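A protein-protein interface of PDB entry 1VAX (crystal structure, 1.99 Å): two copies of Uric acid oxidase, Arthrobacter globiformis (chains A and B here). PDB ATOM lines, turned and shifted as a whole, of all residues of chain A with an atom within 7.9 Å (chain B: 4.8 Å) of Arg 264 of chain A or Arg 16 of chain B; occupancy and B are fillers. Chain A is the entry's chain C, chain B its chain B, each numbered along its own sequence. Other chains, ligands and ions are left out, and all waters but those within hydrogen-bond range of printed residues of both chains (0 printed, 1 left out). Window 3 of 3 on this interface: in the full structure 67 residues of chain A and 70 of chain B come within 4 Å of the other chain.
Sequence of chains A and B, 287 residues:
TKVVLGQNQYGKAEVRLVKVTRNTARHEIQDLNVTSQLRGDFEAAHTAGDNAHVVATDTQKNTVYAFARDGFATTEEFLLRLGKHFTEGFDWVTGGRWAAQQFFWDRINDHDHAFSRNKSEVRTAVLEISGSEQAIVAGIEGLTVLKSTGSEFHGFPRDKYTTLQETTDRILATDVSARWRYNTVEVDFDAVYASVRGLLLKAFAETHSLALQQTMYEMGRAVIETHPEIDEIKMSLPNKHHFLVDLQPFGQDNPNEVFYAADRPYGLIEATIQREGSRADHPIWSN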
ATOM      1  N   HIS A 241     -13.172 -33.428  -6.540  1.00  0.00           N
ATOM      2  CA  HIS A 241     -14.092 -34.551  -6.535  1.00  0.00           C
ATOM      3  C   HIS A 241     -13.546 -35.922  -6.871  1.00  0.00           C
ATOM      4  O   HIS A 241     -12.874 -36.119  -7.884  1.00  0.00           O
ATOM      5  CB  HIS A 241     -15.266 -34.232  -7.457  1.00  0.00           C
ATOM      6  CG  HIS A 241     -15.948 -32.946  -7.116  1.00  0.00           C
ATOM      7  ND1 HIS A 241     -16.208 -31.968  -8.051  1.00  0.00           N
ATOM      8  CD2 HIS A 241     -16.385 -32.458  -5.930  1.00  0.00           C
ATOM      9  CE1 HIS A 241     -16.770 -30.931  -7.456  1.00  0.00           C
ATOM     10  NE2 HIS A 241     -16.889 -31.203  -6.170  1.00  0.00           N
ATOM     11  N   PHE A 243     -15.284 -39.335  -7.326  1.00  0.00           N
ATOM     12  CA  PHE A 243     -16.582 -39.971  -7.479  1.00  0.00           C
ATOM     13  C   PHE A 243     -16.556 -41.464  -7.221  1.00  0.00           C
ATOM     14  O   PHE A 243     -15.739 -42.193  -7.792  1.00  0.00           O
ATOM     15  CB  PHE A 243     -17.119 -39.701  -8.886  1.00  0.00           C
ATOM     16  CG  PHE A 243     -17.386 -38.247  -9.162  1.00  0.00           C
ATOM     17  CD1 PHE A 243     -18.514 -37.621  -8.635  1.00  0.00           C
ATOM     18  CD2 PHE A 243     -16.501 -37.497  -9.935  1.00  0.00           C
ATOM     19  CE1 PHE A 243     -18.758 -36.268  -8.875  1.00  0.00           C
ATOM     20  CE2 PHE A 243     -16.735 -36.146 -10.181  1.00  0.00           C
ATOM     21  CZ  PHE A 243     -17.866 -35.531  -9.651  1.00  0.00           C
ATOM     22  N   TYR A 260     -13.102 -42.363  -8.972  1.00  0.00           N
ATOM     23  CA  TYR A 260     -12.651 -41.699 -10.188  1.00  0.00           C
ATOM     24  C   TYR A 260     -12.285 -40.263  -9.753  1.00  0.00           C
ATOM     25  O   TYR A 260     -13.144 -39.522  -9.282  1.00  0.00           O
ATOM     26  CB  TYR A 260     -13.794 -41.661 -11.204  1.00  0.00           C
ATOM     27  CG  TYR A 260     -13.711 -40.535 -12.218  1.00  0.00           C
ATOM     28  CD1 TYR A 260     -14.837 -39.766 -12.524  1.00  0.00           C
ATOM     29  CD2 TYR A 260     -12.516 -40.240 -12.873  1.00  0.00           C
ATOM     30  CE1 TYR A 260     -14.771 -38.732 -13.458  1.00  0.00           C
ATOM     31  CE2 TYR A 260     -12.439 -39.212 -13.808  1.00  0.00           C
ATOM     32  CZ  TYR A 260     -13.568 -38.463 -14.094  1.00  0.00           C
ATOM     33  OH  TYR A 260     -13.495 -37.451 -15.024  1.00  0.00           O
ATOM     34  N   ALA A 261     -11.021 -39.876  -9.896  1.00  0.00           N
ATOM     35  CA  ALA A 261     -10.595 -38.529  -9.502  1.00  0.00           C
ATOM     36  C   ALA A 261     -10.703 -37.574 -10.691  1.00  0.00           C
ATOM     37  O   ALA A 261      -9.790 -37.491 -11.510  1.00  0.00           O
ATOM     38  CB  ALA A 261      -9.157 -38.567  -8.984  1.00  0.00           C
ATOM     39  N   ALA A 262     -11.822 -36.858 -10.778  1.00  0.00           N
ATOM     40  CA  ALA A 262     -12.076 -35.920 -11.871  1.00  0.00           C
ATOM     41  C   ALA A 262     -11.208 -34.663 -11.803  1.00  0.00           C
ATOM     42  O   ALA A 262     -10.903 -34.165 -10.723  1.00  0.00           O
ATOM     43  CB  ALA A 262     -13.547 -35.526 -11.879  1.00  0.00           C
ATOM     44  N   ASP A 263     -10.819 -34.156 -12.969  1.00  0.00           N
ATOM     45  CA  ASP A 263      -9.980 -32.960 -13.054  1.00  0.00           C
ATOM     46  C   ASP A 263     -10.814 -31.692 -12.880  1.00  0.00           C
ATOM     47  O   ASP A 263     -10.607 -30.920 -11.945  1.00  0.00           O
ATOM     48  CB  ASP A 263      -9.281 -32.914 -14.413  1.00  0.00           C
ATOM     49  CG  ASP A 263      -8.264 -34.025 -14.585  1.00  0.00           C
ATOM     50  OD1 ASP A 263      -7.930 -34.348 -15.743  1.00  0.00           O
ATOM     51  OD2 ASP A 263      -7.789 -34.568 -13.566  1.00  0.00           O
ATOM     52  N   ARG A 264     -11.740 -31.485 -13.808  1.00  0.00           N
ATOM     53  CA  ARG A 264     -12.625 -30.330 -13.799  1.00  0.00           C
ATOM     54  C   ARG A 264     -14.024 -30.822 -14.159  1.00  0.00           C
ATOM     55  O   ARG A 264     -14.175 -31.803 -14.877  1.00  0.00           O
ATOM     56  CB  ARG A 264     -12.159 -29.295 -14.826  1.00  0.00           C
ATOM     57  CG  ARG A 264     -10.745 -28.785 -14.585  1.00  0.00           C
ATOM     58  CD  ARG A 264     -10.363 -27.689 -15.562  1.00  0.00           C
ATOM     59  NE  ARG A 264     -10.309 -28.168 -16.940  1.00  0.00           N
ATOM     60  CZ  ARG A 264     -10.111 -27.381 -17.989  1.00  0.00           C
ATOM     61  NH1 ARG A 264      -9.953 -26.072 -17.817  1.00  0.00           N
ATOM     62  NH2 ARG A 264     -10.061 -27.900 -19.209  1.00  0.00           N
ATOM     63  N   PRO A 265     -15.067 -30.147 -13.656  1.00  0.00           N
ATOM     64  CA  PRO A 265     -14.971 -28.975 -12.786  1.00  0.00           C
ATOM     65  C   PRO A 265     -14.667 -29.380 -11.353  1.00  0.00           C
ATOM     66  O   PRO A 265     -14.609 -30.571 -11.032  1.00  0.00           O
ATOM     67  CB  PRO A 265     -16.353 -28.341 -12.921  1.00  0.00           C
ATOM     68  CG  PRO A 265     -17.244 -29.550 -13.010  1.00  0.00           C
ATOM     69  CD  PRO A 265     -16.475 -30.478 -13.948  1.00  0.00           C
ATOM     70  N   TYR A 266     -14.473 -28.385 -10.496  1.00  0.00           N
ATOM     71  CA  TYR A 266     -14.202 -28.628  -9.089  1.00  0.00           C
ATOM     72  C   TYR A 266     -14.859 -27.535  -8.264  1.00  0.00           C
ATOM     73  O   TYR A 266     -15.053 -26.416  -8.741  1.00  0.00           O
ATOM     74  CB  TYR A 266     -12.690 -28.637  -8.798  1.00  0.00           C
ATOM     75  CG  TYR A 266     -11.932 -27.443  -9.345  1.00  0.00           C
ATOM     76  CD1 TYR A 266     -11.455 -27.443 -10.655  1.00  0.00           C
ATOM     77  CD2 TYR A 266     -11.698 -26.310  -8.558  1.00  0.00           C
ATOM     78  CE1 TYR A 266     -10.764 -26.353 -11.178  1.00  0.00           C
ATOM     79  CE2 TYR A 266     -10.999 -25.199  -9.077  1.00  0.00           C
ATOM     80  CZ  TYR A 266     -10.538 -25.238 -10.388  1.00  0.00           C
ATOM     81  OH  TYR A 266      -9.852 -24.178 -10.929  1.00  0.00           O
ATOM     82  N   GLY A 267     -15.215 -27.866  -7.031  1.00  0.00           N
ATOM     83  CA  GLY A 267     -15.814 -26.865  -6.175  1.00  0.00           C
ATOM     84  C   GLY A 267     -14.671 -25.964  -5.752  1.00  0.00           C
ATOM     85  O   GLY A 267     -13.518 -26.408  -5.689  1.00  0.00           O
ATOM     86  N   GLU B  14     -14.495 -23.774 -13.246  1.00  0.00           N
ATOM     87  CA  GLU B  14     -14.140 -24.393 -14.516  1.00  0.00           C
ATOM     88  C   GLU B  14     -15.069 -25.461 -15.077  1.00  0.00           C
ATOM     89  O   GLU B  14     -14.683 -26.616 -15.283  1.00  0.00           O
ATOM     90  CB  GLU B  14     -12.703 -24.920 -14.435  1.00  0.00           C
ATOM     91  CG  GLU B  14     -11.710 -23.812 -14.077  1.00  0.00           C
ATOM     92  CD  GLU B  14     -10.271 -24.176 -14.385  1.00  0.00           C
ATOM     93  OE1 GLU B  14      -9.490 -24.392 -13.437  1.00  0.00           O
ATOM     94  OE2 GLU B  14      -9.926 -24.249 -15.582  1.00  0.00           O
ATOM     95  N   VAL B  15     -16.306 -25.057 -15.326  1.00  0.00           N
ATOM     96  CA  VAL B  15     -17.274 -25.949 -15.925  1.00  0.00           C
ATOM     97  C   VAL B  15     -17.063 -25.731 -17.420  1.00  0.00           C
ATOM     98  O   VAL B  15     -17.328 -24.646 -17.936  1.00  0.00           O
ATOM     99  CB  VAL B  15     -18.711 -25.563 -15.538  1.00  0.00           C
ATOM    100  CG1 VAL B  15     -19.703 -26.433 -16.303  1.00  0.00           C
ATOM    101  CG2 VAL B  15     -18.902 -25.744 -14.034  1.00  0.00           C
ATOM    102  N   ARG B  16     -16.547 -26.750 -18.104  1.00  0.00           N
ATOM    103  CA  ARG B  16     -16.292 -26.652 -19.538  1.00  0.00           C
ATOM    104  C   ARG B  16     -17.564 -26.944 -20.311  1.00  0.00           C
ATOM    105  O   ARG B  16     -18.118 -28.046 -20.238  1.00  0.00           O
ATOM    106  CB  ARG B  16     -15.174 -27.618 -19.941  1.00  0.00           C
ATOM    107  CG  ARG B  16     -13.814 -27.202 -19.397  1.00  0.00           C
ATOM    108  CD  ARG B  16     -13.211 -26.084 -20.235  1.00  0.00           C
ATOM    109  NE  ARG B  16     -12.811 -26.580 -21.551  1.00  0.00           N
ATOM    110  CZ  ARG B  16     -13.488 -26.378 -22.677  1.00  0.00           C
ATOM    111  NH1 ARG B  16     -13.035 -26.887 -23.815  1.00  0.00           N
ATOM    112  NH2 ARG B  16     -14.604 -25.652 -22.674  1.00  0.00           N
ATOM    113  N   LEU B  17     -18.008 -25.943 -21.062  1.00  0.00           N
ATOM    114  CA  LEU B  17     -19.226 -26.035 -21.840  1.00  0.00           C
ATOM    115  C   LEU B  17     -19.024 -25.733 -23.319  1.00  0.00           C
ATOM    116  O   LEU B  17     -18.319 -24.793 -23.698  1.00  0.00           O
ATOM    117  CB  LEU B  17     -20.265 -25.063 -21.250  1.00  0.00           C
ATOM    118  CG  LEU B  17     -21.596 -24.739 -21.945  1.00  0.00           C
ATOM    119  CD1 LEU B  17     -21.356 -23.884 -23.163  1.00  0.00           C
ATOM    120  CD2 LEU B  17     -22.329 -26.010 -22.313  1.00  0.00           C
ATOM    121  N   VAL B  18     -19.634 -26.560 -24.154  1.00  0.00           N
ATOM    122  CA  VAL B  18     -19.593 -26.349 -25.586  1.00  0.00           C
ATOM    123  C   VAL B  18     -21.054 -26.339 -26.008  1.00  0.00           C
ATOM    124  O   VAL B  18     -21.791 -27.301 -25.774  1.00  0.00           O
ATOM    125  CB  VAL B  18     -18.827 -27.459 -26.326  1.00  0.00           C
ATOM    126  CG1 VAL B  18     -19.001 -27.294 -27.837  1.00  0.00           C
ATOM    127  CG2 VAL B  18     -17.344 -27.379 -25.973  1.00  0.00           C
ATOM    128  N   ASP B  31     -17.659 -22.118 -27.115  1.00  0.00           N
ATOM    129  CA  ASP B  31     -16.839 -22.900 -26.201  1.00  0.00           C
ATOM    130  C   ASP B  31     -16.456 -22.036 -25.001  1.00  0.00           C
ATOM    131  O   ASP B  31     -15.743 -21.036 -25.153  1.00  0.00           O
ATOM    132  CB  ASP B  31     -15.587 -23.356 -26.957  1.00  0.00           C
ATOM    133  CG  ASP B  31     -14.825 -24.451 -26.240  1.00  0.00           C
ATOM    134  OD1 ASP B  31     -14.974 -24.582 -25.007  1.00  0.00           O
ATOM    135  OD2 ASP B  31     -14.057 -25.171 -26.918  1.00  0.00           O
ATOM    136  N   LEU B  32     -16.921 -22.428 -23.816  1.00  0.00           N
ATOM    137  CA  LEU B  32     -16.659 -21.661 -22.599  1.00  0.00           C
ATOM    138  C   LEU B  32     -16.134 -22.467 -21.416  1.00  0.00           C
ATOM    139  O   LEU B  32     -16.353 -23.676 -21.310  1.00  0.00           O
ATOM    140  CB  LEU B  32     -17.945 -20.947 -22.140  1.00  0.00           C
ATOM    141  CG  LEU B  32     -18.731 -20.048 -23.102  1.00  0.00           C
ATOM    142  CD1 LEU B  32     -20.010 -19.566 -22.412  1.00  0.00           C
ATOM    143  CD2 LEU B  32     -17.880 -18.866 -23.529  1.00  0.00           C
ATOM    144  N   ASN B  33     -15.442 -21.766 -20.522  1.00  0.00           N
ATOM    145  CA  ASN B  33     -14.917 -22.339 -19.292  1.00  0.00           C
ATOM    146  C   ASN B  33     -15.566 -21.437 -18.245  1.00  0.00           C
ATOM    147  O   ASN B  33     -15.116 -20.306 -18.023  1.00  0.00           O
ATOM    148  CB  ASN B  33     -13.394 -22.202 -19.227  1.00  0.00           C
ATOM    149  CG  ASN B  33     -12.792 -22.984 -18.079  1.00  0.00           C
ATOM    150  OD1 ASN B  33     -11.643 -22.758 -17.692  1.00  0.00           O
ATOM    151  ND2 ASN B  33     -13.565 -23.920 -17.530  1.00  0.00           N
ATOM    152  N   TYR B  65     -25.394 -25.831 -17.327  1.00  0.00           N
ATOM    153  CA  TYR B  65     -25.776 -26.617 -18.495  1.00  0.00           C
ATOM    154  C   TYR B  65     -27.253 -26.452 -18.858  1.00  0.00           C
ATOM    155  O   TYR B  65     -27.603 -26.374 -20.034  1.00  0.00           O
ATOM    156  CB  TYR B  65     -25.443 -28.095 -18.267  1.00  0.00           C
ATOM    157  CG  TYR B  65     -23.947 -28.366 -18.235  1.00  0.00           C
ATOM    158  CD1 TYR B  65     -23.148 -28.074 -19.336  1.00  0.00           C
ATOM    159  CD2 TYR B  65     -23.335 -28.886 -17.096  1.00  0.00           C
ATOM    160  CE1 TYR B  65     -21.770 -28.291 -19.308  1.00  0.00           C
ATOM    161  CE2 TYR B  65     -21.955 -29.108 -17.055  1.00  0.00           C
ATOM    162  CZ  TYR B  65     -21.182 -28.804 -18.165  1.00  0.00           C
ATOM    163  OH  TYR B  65     -19.819 -28.994 -18.130  1.00  0.00           O
ATOM    164  N   PHE B 103     -13.267 -19.630 -25.784  1.00  0.00           N
ATOM    165  CA  PHE B 103     -12.282 -20.145 -26.725  1.00  0.00           C
ATOM    166  C   PHE B 103     -12.846 -20.060 -28.133  1.00  0.00           C
ATOM    167  O   PHE B 103     -13.991 -20.445 -28.372  1.00  0.00           O
ATOM    168  CB  PHE B 103     -11.939 -21.592 -26.366  1.00  0.00           C
ATOM    169  CG  PHE B 103     -11.556 -21.771 -24.930  1.00  0.00           C
ATOM    170  CD1 PHE B 103     -12.385 -22.462 -24.055  1.00  0.00           C
ATOM    171  CD2 PHE B 103     -10.381 -21.208 -24.437  1.00  0.00           C
ATOM    172  CE1 PHE B 103     -12.052 -22.589 -22.708  1.00  0.00           C
ATOM    173  CE2 PHE B 103     -10.038 -21.329 -23.092  1.00  0.00           C
ATOM    174  CZ  PHE B 103     -10.875 -22.020 -22.227  1.00  0.00           C
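Printed residues of chain B that touch a printed residue of chain A: Glu 14, Val 15, Arg 16 and Asn 33.
Of the 10 printed residues of chain A, 3 touch a printed residue of chain B.
Along chain A the printed residues that touch a printed residue of chain B span positions 264 to 266.
Among the printed residues, Asp or Glu carboxylates within 4 Å of a Lys or Arg side-chain nitrogen of the other chain: Arg 264 of chain A with Glu 14 of chain B.
No position is printed for both chains.
Of the 6 pairs that touch across the chains among the printed residues, none has its exchanged pair printed and touching as well.
OD1 of Asn 33 of chain B sits close to OE2 of Glu 14 of chain B (3.1 Å).
The guanidinium group (NH2) of Arg 16 of chain B lies within salt-bridge range of the side-chain carboxylate (OD1) of Asp 31 of chain B (2.6 Å).
O of Leu 32 of chain B is in hydrogen-bond range of NH2 of Arg 16 of chain B.
The backbone carbonyl oxygen (O) of Arg 16 of chain B sits at hydrogen-bond distance from the side-chain hydroxyl (OH) of Tyr 65 of chain B.
NH1 of Arg 264 of chain A is in salt-bridge range of OE2 of Glu 14 of chain B (2.9 Å).
The side-chain carboxylate of Glu 14 of chain B is in hydrogen-bond range of the side-chain hydroxyl of Tyr 266 of chain A.
Among the printed residues, merely in contact across the chains: Pro 265 of chain A with Glu 14 of chain B (3.4 Å), Arg 264 of chain A with Asn 33 of chain B (3.7 Å), Arg 264 of chain A with Arg 16 of chain B (3.8 Å) and Pro 265 of chain A with Val 15 of chain B (3.8 Å).
Arg 16 of chain B touches just one residue of chain A: Arg 264.
Of the printed residues of chain B, Pro 265 of chain A touches Glu 14 (3.4 Å) and Val 15 (3.8 Å).
Of the printed residues of chain A, Asn 33 of chain B touches Arg 264.
Printed residues of chain A within 4 Å of Val 15 of chain B: Pro 265 (3.8 Å).
Printed residues of chain A within 4 Å of Glu 14 of chain B: Arg 264 (2.9 Å), Pro 265 (3.4 Å) and Tyr 266 (2.5 Å).
Printed residues of chain B within 4 Å of Tyr 266 of chain A: Glu 14.
Leu 32 of chain B touches none of the printed residues of chain A.
Ala 262 of chain A touches none of the printed residues of chain B.
The nearest printed residue of chain A that does not touch Val 15 of chain B is Arg 264 of chain A (6.0 Å).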
